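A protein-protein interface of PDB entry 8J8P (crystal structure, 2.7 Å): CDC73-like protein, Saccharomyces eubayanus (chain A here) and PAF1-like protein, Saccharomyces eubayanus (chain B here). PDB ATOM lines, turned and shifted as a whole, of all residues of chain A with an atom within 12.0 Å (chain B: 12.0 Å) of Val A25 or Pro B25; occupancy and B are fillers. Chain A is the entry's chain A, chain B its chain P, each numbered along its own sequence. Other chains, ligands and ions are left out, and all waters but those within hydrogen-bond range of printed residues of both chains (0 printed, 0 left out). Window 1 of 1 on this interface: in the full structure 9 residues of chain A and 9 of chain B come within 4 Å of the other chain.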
ATOM      1  N   THR A  18     -12.539  -6.595 -16.170  1.00  0.00           N
ATOM      2  CA  THR A  18     -12.504  -6.955 -14.771  1.00  0.00           C
ATOM      3  C   THR A  18     -11.950  -5.764 -14.001  1.00  0.00           C
ATOM      4  O   THR A  18     -12.444  -5.446 -12.919  1.00  0.00           O
ATOM      5  CB  THR A  18     -11.613  -8.184 -14.521  1.00  0.00           C
ATOM      6  OG1 THR A  18     -12.374  -9.380 -14.737  1.00  0.00           O
ATOM      7  CG2 THR A  18     -11.084  -8.176 -13.094  1.00  0.00           C
ATOM      8  N   MET A  19     -10.926  -5.099 -14.544  1.00  0.00           N
ATOM      9  CA  MET A  19     -10.413  -3.968 -13.837  1.00  0.00           C
ATOM     10  C   MET A  19     -11.522  -2.973 -13.536  1.00  0.00           C
ATOM     11  O   MET A  19     -11.608  -2.539 -12.410  1.00  0.00           O
ATOM     12  CB  MET A  19      -9.217  -3.312 -14.604  1.00  0.00           C
ATOM     13  CG  MET A  19      -9.394  -1.893 -15.202  1.00  0.00           C
ATOM     14  SD  MET A  19      -7.984  -1.095 -16.038  1.00  0.00           S
ATOM     15  CE  MET A  19      -8.707   0.369 -16.737  1.00  0.00           C
ATOM     16  N   ASN A  21     -15.081  -3.312 -13.444  1.00  0.00           N
ATOM     17  CA  ASN A  21     -16.363  -3.805 -12.924  1.00  0.00           C
ATOM     18  C   ASN A  21     -16.392  -4.358 -11.486  1.00  0.00           C
ATOM     19  O   ASN A  21     -17.470  -4.602 -10.944  1.00  0.00           O
ATOM     20  CB  ASN A  21     -16.950  -4.848 -13.883  1.00  0.00           C
ATOM     21  CG  ASN A  21     -17.643  -4.218 -15.075  1.00  0.00           C
ATOM     22  OD1 ASN A  21     -18.814  -4.486 -15.340  1.00  0.00           O
ATOM     23  ND2 ASN A  21     -16.918  -3.374 -15.802  1.00  0.00           N
ATOM     24  N   GLU A  22     -15.230  -4.555 -10.870  1.00  0.00           N
ATOM     25  CA  GLU A  22     -15.166  -5.069  -9.508  1.00  0.00           C
ATOM     26  C   GLU A  22     -14.851  -3.930  -8.547  1.00  0.00           C
ATOM     27  O   GLU A  22     -13.997  -3.086  -8.832  1.00  0.00           O
ATOM     28  CB  GLU A  22     -14.116  -6.177  -9.371  1.00  0.00           C
ATOM     29  CG  GLU A  22     -12.767  -5.845  -9.984  1.00  0.00           C
ATOM     30  CD  GLU A  22     -11.642  -6.697  -9.422  1.00  0.00           C
ATOM     31  OE1 GLU A  22     -11.897  -7.863  -9.053  1.00  0.00           O
ATOM     32  OE2 GLU A  22     -10.494  -6.203  -9.352  1.00  0.00           O
ATOM     33  N   ARG A  23     -15.554  -3.904  -7.417  1.00  0.00           N
ATOM     34  CA  ARG A  23     -15.402  -2.866  -6.408  1.00  0.00           C
ATOM     35  C   ARG A  23     -14.855  -3.469  -5.120  1.00  0.00           C
ATOM     36  O   ARG A  23     -15.025  -4.662  -4.850  1.00  0.00           O
ATOM     37  CB  ARG A  23     -16.734  -2.158  -6.126  1.00  0.00           C
ATOM     38  CG  ARG A  23     -17.730  -2.162  -7.285  1.00  0.00           C
ATOM     39  CD  ARG A  23     -18.907  -1.237  -6.990  1.00  0.00           C
ATOM     40  NE  ARG A  23     -20.006  -1.925  -6.309  1.00  0.00           N
ATOM     41  CZ  ARG A  23     -21.212  -1.400  -6.119  1.00  0.00           C
ATOM     42  NH1 ARG A  23     -21.476  -0.174  -6.554  1.00  0.00           N
ATOM     43  NH2 ARG A  23     -22.155  -2.095  -5.496  1.00  0.00           N
ATOM     44  N   VAL A  24     -14.205  -2.628  -4.320  1.00  0.00           N
ATOM     45  CA  VAL A  24     -13.524  -3.081  -3.110  1.00  0.00           C
ATOM     46  C   VAL A  24     -14.532  -3.173  -1.968  1.00  0.00           C
ATOM     47  O   VAL A  24     -15.089  -2.161  -1.534  1.00  0.00           O
ATOM     48  CB  VAL A  24     -12.354  -2.155  -2.743  1.00  0.00           C
ATOM     49  CG1 VAL A  24     -11.123  -2.534  -3.548  1.00  0.00           C
ATOM     50  CG2 VAL A  24     -12.724  -0.694  -2.984  1.00  0.00           C
ATOM     51  N   VAL A  25     -14.758  -4.397  -1.479  1.00  0.00           N
ATOM     52  CA  VAL A  25     -15.718  -4.599  -0.399  1.00  0.00           C
ATOM     53  C   VAL A  25     -15.200  -3.982   0.896  1.00  0.00           C
ATOM     54  O   VAL A  25     -15.959  -3.347   1.643  1.00  0.00           O
ATOM     55  CB  VAL A  25     -16.022  -6.101  -0.241  1.00  0.00           C
ATOM     56  CG1 VAL A  25     -14.739  -6.908  -0.248  1.00  0.00           C
ATOM     57  CG2 VAL A  25     -16.832  -6.351   1.027  1.00  0.00           C
ATOM     58  N   GLN A  26     -13.901  -4.132   1.171  1.00  0.00           N
ATOM     59  CA  GLN A  26     -13.299  -3.645   2.409  1.00  0.00           C
ATOM     60  C   GLN A  26     -11.820  -3.425   2.150  1.00  0.00           C
ATOM     61  O   GLN A  26     -11.133  -4.344   1.699  1.00  0.00           O
ATOM     62  CB  GLN A  26     -13.515  -4.647   3.541  1.00  0.00           C
ATOM     63  CG  GLN A  26     -13.774  -4.031   4.910  1.00  0.00           C
ATOM     64  CD  GLN A  26     -13.892  -5.091   5.991  1.00  0.00           C
ATOM     65  OE1 GLN A  26     -14.408  -4.836   7.083  1.00  0.00           O
ATOM     66  NE2 GLN A  26     -13.424  -6.295   5.684  1.00  0.00           N
ATOM     67  N   ASP A  27     -11.332  -2.223   2.443  1.00  0.00           N
ATOM     68  CA  ASP A  27      -9.935  -1.903   2.195  1.00  0.00           C
ATOM     69  C   ASP A  27      -9.027  -2.708   3.128  1.00  0.00           C
ATOM     70  O   ASP A  27      -9.482  -3.456   4.000  1.00  0.00           O
ATOM     71  CB  ASP A  27      -9.684  -0.404   2.377  1.00  0.00           C
ATOM     72  CG  ASP A  27     -10.787   0.451   1.775  1.00  0.00           C
ATOM     73  OD1 ASP A  27     -10.545   1.094   0.730  1.00  0.00           O
ATOM     74  OD2 ASP A  27     -11.898   0.474   2.348  1.00  0.00           O
ATOM     75  N   HIS A  28      -7.717  -2.556   2.925  1.00  0.00           N
ATOM     76  CA  HIS A  28      -6.753  -3.146   3.848  1.00  0.00           C
ATOM     77  C   HIS A  28      -6.627  -2.329   5.126  1.00  0.00           C
ATOM     78  O   HIS A  28      -6.252  -2.872   6.172  1.00  0.00           O
ATOM     79  CB  HIS A  28      -5.387  -3.262   3.180  1.00  0.00           C
ATOM     80  CG  HIS A  28      -4.660  -1.959   3.081  1.00  0.00           C
ATOM     81  ND1 HIS A  28      -3.331  -1.818   3.421  1.00  0.00           N
ATOM     82  CD2 HIS A  28      -5.078  -0.734   2.681  1.00  0.00           C
ATOM     83  CE1 HIS A  28      -2.963  -0.564   3.234  1.00  0.00           C
ATOM     84  NE2 HIS A  28      -4.003   0.115   2.784  1.00  0.00           N
ATOM     85  N   ASN A  29      -6.919  -1.033   5.056  1.00  0.00           N
ATOM     86  CA  ASN A  29      -6.914  -0.149   6.209  1.00  0.00           C
ATOM     87  C   ASN A  29      -8.254  -0.118   6.925  1.00  0.00           C
ATOM     88  O   ASN A  29      -8.377   0.556   7.953  1.00  0.00           O
ATOM     89  CB  ASN A  29      -6.537   1.270   5.779  1.00  0.00           C
ATOM     90  CG  ASN A  29      -5.045   1.478   5.728  1.00  0.00           C
ATOM     91  OD1 ASN A  29      -4.468   1.699   4.664  1.00  0.00           O
ATOM     92  ND2 ASN A  29      -4.406   1.392   6.881  1.00  0.00           N
ATOM     93  N   SER A  30      -9.258  -0.825   6.406  1.00  0.00           N
ATOM     94  CA  SER A  30     -10.595  -0.792   6.968  1.00  0.00           C
ATOM     95  C   SER A  30     -11.078  -2.134   7.502  1.00  0.00           C
ATOM     96  O   SER A  30     -12.089  -2.164   8.211  1.00  0.00           O
ATOM     97  CB  SER A  30     -11.597  -0.267   5.925  1.00  0.00           C
ATOM     98  OG  SER A  30     -11.752  -1.175   4.850  1.00  0.00           O
ATOM     99  N   ALA A  31     -10.399  -3.237   7.196  1.00  0.00           N
ATOM    100  CA  ALA A  31     -10.728  -4.518   7.809  1.00  0.00           C
ATOM    101  C   ALA A  31      -9.908  -4.791   9.063  1.00  0.00           C
ATOM    102  O   ALA A  31      -9.988  -5.893   9.619  1.00  0.00           O
ATOM    103  CB  ALA A  31     -10.543  -5.658   6.808  1.00  0.00           C
ATOM    104  N   LEU A  32      -9.127  -3.810   9.516  1.00  0.00           N
ATOM    105  CA  LEU A  32      -8.379  -3.894  10.763  1.00  0.00           C
ATOM    106  C   LEU A  32      -9.278  -3.563  11.949  1.00  0.00           C
ATOM    107  O   LEU A  32      -8.829  -2.928  12.907  1.00  0.00           O
ATOM    108  CB  LEU A  32      -7.194  -2.923  10.738  1.00  0.00           C
ATOM    109  CG  LEU A  32      -6.230  -2.944   9.554  1.00  0.00           C
ATOM    110  CD1 LEU A  32      -5.435  -1.645   9.498  1.00  0.00           C
ATOM    111  CD2 LEU A  32      -5.297  -4.135   9.654  1.00  0.00           C
ATOM    112  N   ARG A  33     -10.553  -3.963  11.896  1.00  0.00           N
ATOM    113  CA  ARG A  33     -11.532  -3.467  12.857  1.00  0.00           C
ATOM    114  C   ARG A  33     -12.380  -4.563  13.495  1.00  0.00           C
ATOM    115  O   ARG A  33     -13.326  -4.244  14.225  1.00  0.00           O
ATOM    116  CB  ARG A  33     -12.442  -2.429  12.189  1.00  0.00           C
ATOM    117  CG  ARG A  33     -11.680  -1.330  11.463  1.00  0.00           C
ATOM    118  CD  ARG A  33     -12.550  -0.122  11.173  1.00  0.00           C
ATOM    119  NE  ARG A  33     -12.999  -0.094   9.783  1.00  0.00           N
ATOM    120  CZ  ARG A  33     -13.450   0.993   9.168  1.00  0.00           C
ATOM    121  NH1 ARG A  33     -13.504   2.148   9.818  1.00  0.00           N
ATOM    122  NH2 ARG A  33     -13.843   0.931   7.902  1.00  0.00           N
ATOM    123  N   GLY A  34     -12.073  -5.833  13.258  1.00  0.00           N
ATOM    124  CA  GLY A  34     -12.821  -6.895  13.898  1.00  0.00           C
ATOM    125  C   GLY A  34     -14.113  -7.223  13.181  1.00  0.00           C
ATOM    126  O   GLY A  34     -14.142  -7.272  11.949  1.00  0.00           O
ATOM    127  N   VAL B  20      -2.810 -10.833   8.614  1.00  0.00           N
ATOM    128  CA  VAL B  20      -2.331 -10.982   7.242  1.00  0.00           C
ATOM    129  C   VAL B  20      -3.076  -9.993   6.350  1.00  0.00           C
ATOM    130  O   VAL B  20      -4.276  -9.771   6.570  1.00  0.00           O
ATOM    131  CB  VAL B  20      -2.502 -12.437   6.770  1.00  0.00           C
ATOM    132  CG1 VAL B  20      -3.917 -12.957   7.075  1.00  0.00           C
ATOM    133  CG2 VAL B  20      -2.126 -12.584   5.296  1.00  0.00           C
ATOM    134  N   PRO B  21      -2.420  -9.333   5.358  1.00  0.00           N
ATOM    135  CA  PRO B  21      -3.175  -8.429   4.468  1.00  0.00           C
ATOM    136  C   PRO B  21      -4.324  -9.121   3.738  1.00  0.00           C
ATOM    137  O   PRO B  21      -4.139 -10.027   2.921  1.00  0.00           O
ATOM    138  CB  PRO B  21      -2.104  -7.885   3.509  1.00  0.00           C
ATOM    139  CG  PRO B  21      -0.908  -8.758   3.681  1.00  0.00           C
ATOM    140  CD  PRO B  21      -0.968  -9.274   5.106  1.00  0.00           C
ATOM    141  N   GLN B  22      -5.531  -8.684   4.076  1.00  0.00           N
ATOM    142  CA  GLN B  22      -6.785  -9.283   3.645  1.00  0.00           C
ATOM    143  C   GLN B  22      -7.234  -8.657   2.332  1.00  0.00           C
ATOM    144  O   GLN B  22      -7.287  -7.430   2.202  1.00  0.00           O
ATOM    145  CB  GLN B  22      -7.860  -9.099   4.722  1.00  0.00           C
ATOM    146  CG  GLN B  22      -8.274  -7.638   5.033  1.00  0.00           C
ATOM    147  CD  GLN B  22      -7.138  -6.713   5.527  1.00  0.00           C
ATOM    148  OE1 GLN B  22      -5.951  -6.990   5.353  1.00  0.00           O
ATOM    149  NE2 GLN B  22      -7.521  -5.594   6.133  1.00  0.00           N
ATOM    150  N   LEU B  23      -7.548  -9.503   1.355  1.00  0.00           N
ATOM    151  CA  LEU B  23      -8.125  -9.075   0.080  1.00  0.00           C
ATOM    152  C   LEU B  23      -9.405  -9.885  -0.119  1.00  0.00           C
ATOM    153  O   LEU B  23      -9.385 -10.948  -0.760  1.00  0.00           O
ATOM    154  CB  LEU B  23      -7.159  -9.272  -1.091  1.00  0.00           C
ATOM    155  CG  LEU B  23      -5.785  -8.582  -1.101  1.00  0.00           C
ATOM    156  CD1 LEU B  23      -5.867  -7.152  -0.570  1.00  0.00           C
ATOM    157  CD2 LEU B  23      -4.745  -9.399  -0.349  1.00  0.00           C
ATOM    158  N   PRO B  24     -10.530  -9.424   0.427  1.00  0.00           N
ATOM    159  CA  PRO B  24     -11.753 -10.246   0.430  1.00  0.00           C
ATOM    160  C   PRO B  24     -12.321 -10.385  -0.969  1.00  0.00           C
ATOM    161  O   PRO B  24     -11.924  -9.642  -1.881  1.00  0.00           O
ATOM    162  CB  PRO B  24     -12.711  -9.452   1.341  1.00  0.00           C
ATOM    163  CG  PRO B  24     -11.872  -8.381   1.993  1.00  0.00           C
ATOM    164  CD  PRO B  24     -10.757  -8.108   1.040  1.00  0.00           C
ATOM    165  N   PRO B  25     -13.240 -11.330  -1.183  1.00  0.00           N
ATOM    166  CA  PRO B  25     -13.902 -11.442  -2.489  1.00  0.00           C
ATOM    167  C   PRO B  25     -14.509 -10.114  -2.923  1.00  0.00           C
ATOM    168  O   PRO B  25     -15.106  -9.389  -2.123  1.00  0.00           O
ATOM    169  CB  PRO B  25     -14.978 -12.506  -2.246  1.00  0.00           C
ATOM    170  CG  PRO B  25     -14.429 -13.344  -1.149  1.00  0.00           C
ATOM    171  CD  PRO B  25     -13.666 -12.397  -0.259  1.00  0.00           C
ATOM    172  N   LYS B  26     -14.359  -9.799  -4.205  1.00  0.00           N
ATOM    173  CA  LYS B  26     -14.678  -8.472  -4.707  1.00  0.00           C
ATOM    174  C   LYS B  26     -16.143  -8.367  -5.119  1.00  0.00           C
ATOM    175  O   LYS B  26     -16.706  -9.286  -5.723  1.00  0.00           O
ATOM    176  CB  LYS B  26     -13.769  -8.124  -5.885  1.00  0.00           C
ATOM    177  CG  LYS B  26     -12.326  -8.586  -5.697  1.00  0.00           C
ATOM    178  CD  LYS B  26     -11.336  -7.452  -5.934  1.00  0.00           C
ATOM    179  CE  LYS B  26      -9.899  -7.900  -5.701  1.00  0.00           C
ATOM    180  NZ  LYS B  26      -9.188  -7.016  -4.730  1.00  0.00           N
ATOM    181  N   LEU B  27     -16.757  -7.238  -4.766  1.00  0.00           N
ATOM    182  CA  LEU B  27     -18.077  -6.884  -5.266  1.00  0.00           C
ATOM    183  C   LEU B  27     -17.987  -6.501  -6.738  1.00  0.00           C
ATOM    184  O   LEU B  27     -17.005  -5.893  -7.172  1.00  0.00           O
ATOM    185  CB  LEU B  27     -18.656  -5.715  -4.465  1.00  0.00           C
ATOM    186  CG  LEU B  27     -19.681  -5.990  -3.362  1.00  0.00           C
ATOM    187  CD1 LEU B  27     -19.015  -6.557  -2.125  1.00  0.00           C
ATOM    188  CD2 LEU B  27     -20.485  -4.739  -3.024  1.00  0.00           C
ATOM    189  N   LEU B  28     -19.013  -6.858  -7.509  1.00  0.00           N
ATOM    190  CA  LEU B  28     -19.144  -6.393  -8.882  1.00  0.00           C
ATOM    191  C   LEU B  28     -20.242  -5.341  -8.995  1.00  0.00           C
ATOM    192  O   LEU B  28     -21.236  -5.370  -8.263  1.00  0.00           O
ATOM    193  CB  LEU B  28     -19.456  -7.533  -9.856  1.00  0.00           C
ATOM    194  CG  LEU B  28     -18.603  -8.793  -9.854  1.00  0.00           C
ATOM    195  CD1 LEU B  28     -19.414  -9.931  -9.319  1.00  0.00           C
ATOM    196  CD2 LEU B  28     -18.106  -9.094 -11.254  1.00  0.00           C
ATOM    197  N   ALA B  29     -20.051  -4.410  -9.928  1.00  0.00           N
ATOM    198  CA  ALA B  29     -21.095  -3.456 -10.263  1.00  0.00           C
ATOM    199  C   ALA B  29     -22.174  -4.135 -11.103  1.00  0.00           C
ATOM    200  O   ALA B  29     -21.938  -5.150 -11.765  1.00  0.00           O
ATOM    201  CB  ALA B  29     -20.514  -2.256 -11.011  1.00  0.00           C
ATOM    202  N   TYR B  30     -23.373  -3.556 -11.068  1.00  0.00           N
ATOM    203  CA  TYR B  30     -24.515  -4.148 -11.756  1.00  0.00           C
ATOM    204  C   TYR B  30     -24.599  -3.639 -13.194  1.00  0.00           C
ATOM    205  O   TYR B  30     -24.253  -2.485 -13.466  1.00  0.00           O
ATOM    206  CB  TYR B  30     -25.806  -3.823 -11.014  1.00  0.00           C
ATOM    207  CG  TYR B  30     -25.704  -4.063  -9.525  1.00  0.00           C
ATOM    208  CD1 TYR B  30     -25.308  -3.050  -8.661  1.00  0.00           C
ATOM    209  CD2 TYR B  30     -25.989  -5.312  -8.983  1.00  0.00           C
ATOM    210  CE1 TYR B  30     -25.203  -3.272  -7.295  1.00  0.00           C
ATOM    211  CE2 TYR B  30     -25.890  -5.544  -7.620  1.00  0.00           C
ATOM    212  CZ  TYR B  30     -25.496  -4.523  -6.780  1.00  0.00           C
ATOM    213  OH  TYR B  30     -25.396  -4.754  -5.423  1.00  0.00           O
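The backbone NH of Ala B29 lies within hydrogen-bond range of the backbone carbonyl oxygen of Asn A21 (2.8 Å). The backbone NH (N) of Arg A23 sits at hydrogen-bond distance from the backbone carbonyl oxygen (O) of Leu B27 (2.5 Å). O of His A28 sits at hydrogen-bond distance from NE2 of Gln B22, at 3.0 Å.
OG of Ser A30 sits at hydrogen-bond distance from N of Asp A27. A ring nitrogen (NE2) of His A28 lies within hydrogen-bond range of the side-chain amide oxygen (OD1) of Asn A29. O of Val B20 lies close to OE1 of Gln B22 (3.5 Å).
Among the printed residues, merely in contact across the chains: Glu A22 with Leu B27, Ala A31 with Gln B22, Val A25 with Pro B25, Glu A22 with Lys B26, Asn A21 with Leu B28, Val A25 with Leu B27, Asp A27 with Gln B22, Val A25 with Pro B24, Arg A23 with Tyr B30, Arg A23 with Lys B26 and Gln A26 with Pro B24.
Val A25 touches just these residues of chain B: Pro B24 (3.6 Å), Pro B25 (3.1 Å) and Leu B27 (3.6 Å). Gln A26 touches one residue of chain B. Of chain B, only Gln B22 comes within 4 Å of Asp A27. Pro B24 touches just these residues of chain A: Val A25 (3.6 Å) and Gln A26 (3.8 Å). Lys B26 touches just these residues of chain A: Glu A22 and Arg A23. Printed residues of chain B within 4 Å of Glu A22: Lys B26 (3.2 Å) and Leu B27 (3.1 Å). Of the printed residues of chain A, Gln B22 touches Asp A27, His A28 and Ala A31. Of the printed residues of chain A, Tyr B30 touches Arg A23. Of the printed residues of chain B, Asn A21 touches Leu B28 (3.2 Å) and Ala B29 (2.8 Å). Asn A29 touches none of the printed residues of chain B. Leu B23 touches none of the printed residues of chain A. The nearest residue of chain B that does not touch Val A25 is Lys B26 (4.7 Å). The nearest residue of chain A that does not touch Pro B25 is Arg A23 (5.5 Å). The nearest printed residue of chain B that does not touch Ala A31 is Pro B24 (5.7 Å).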
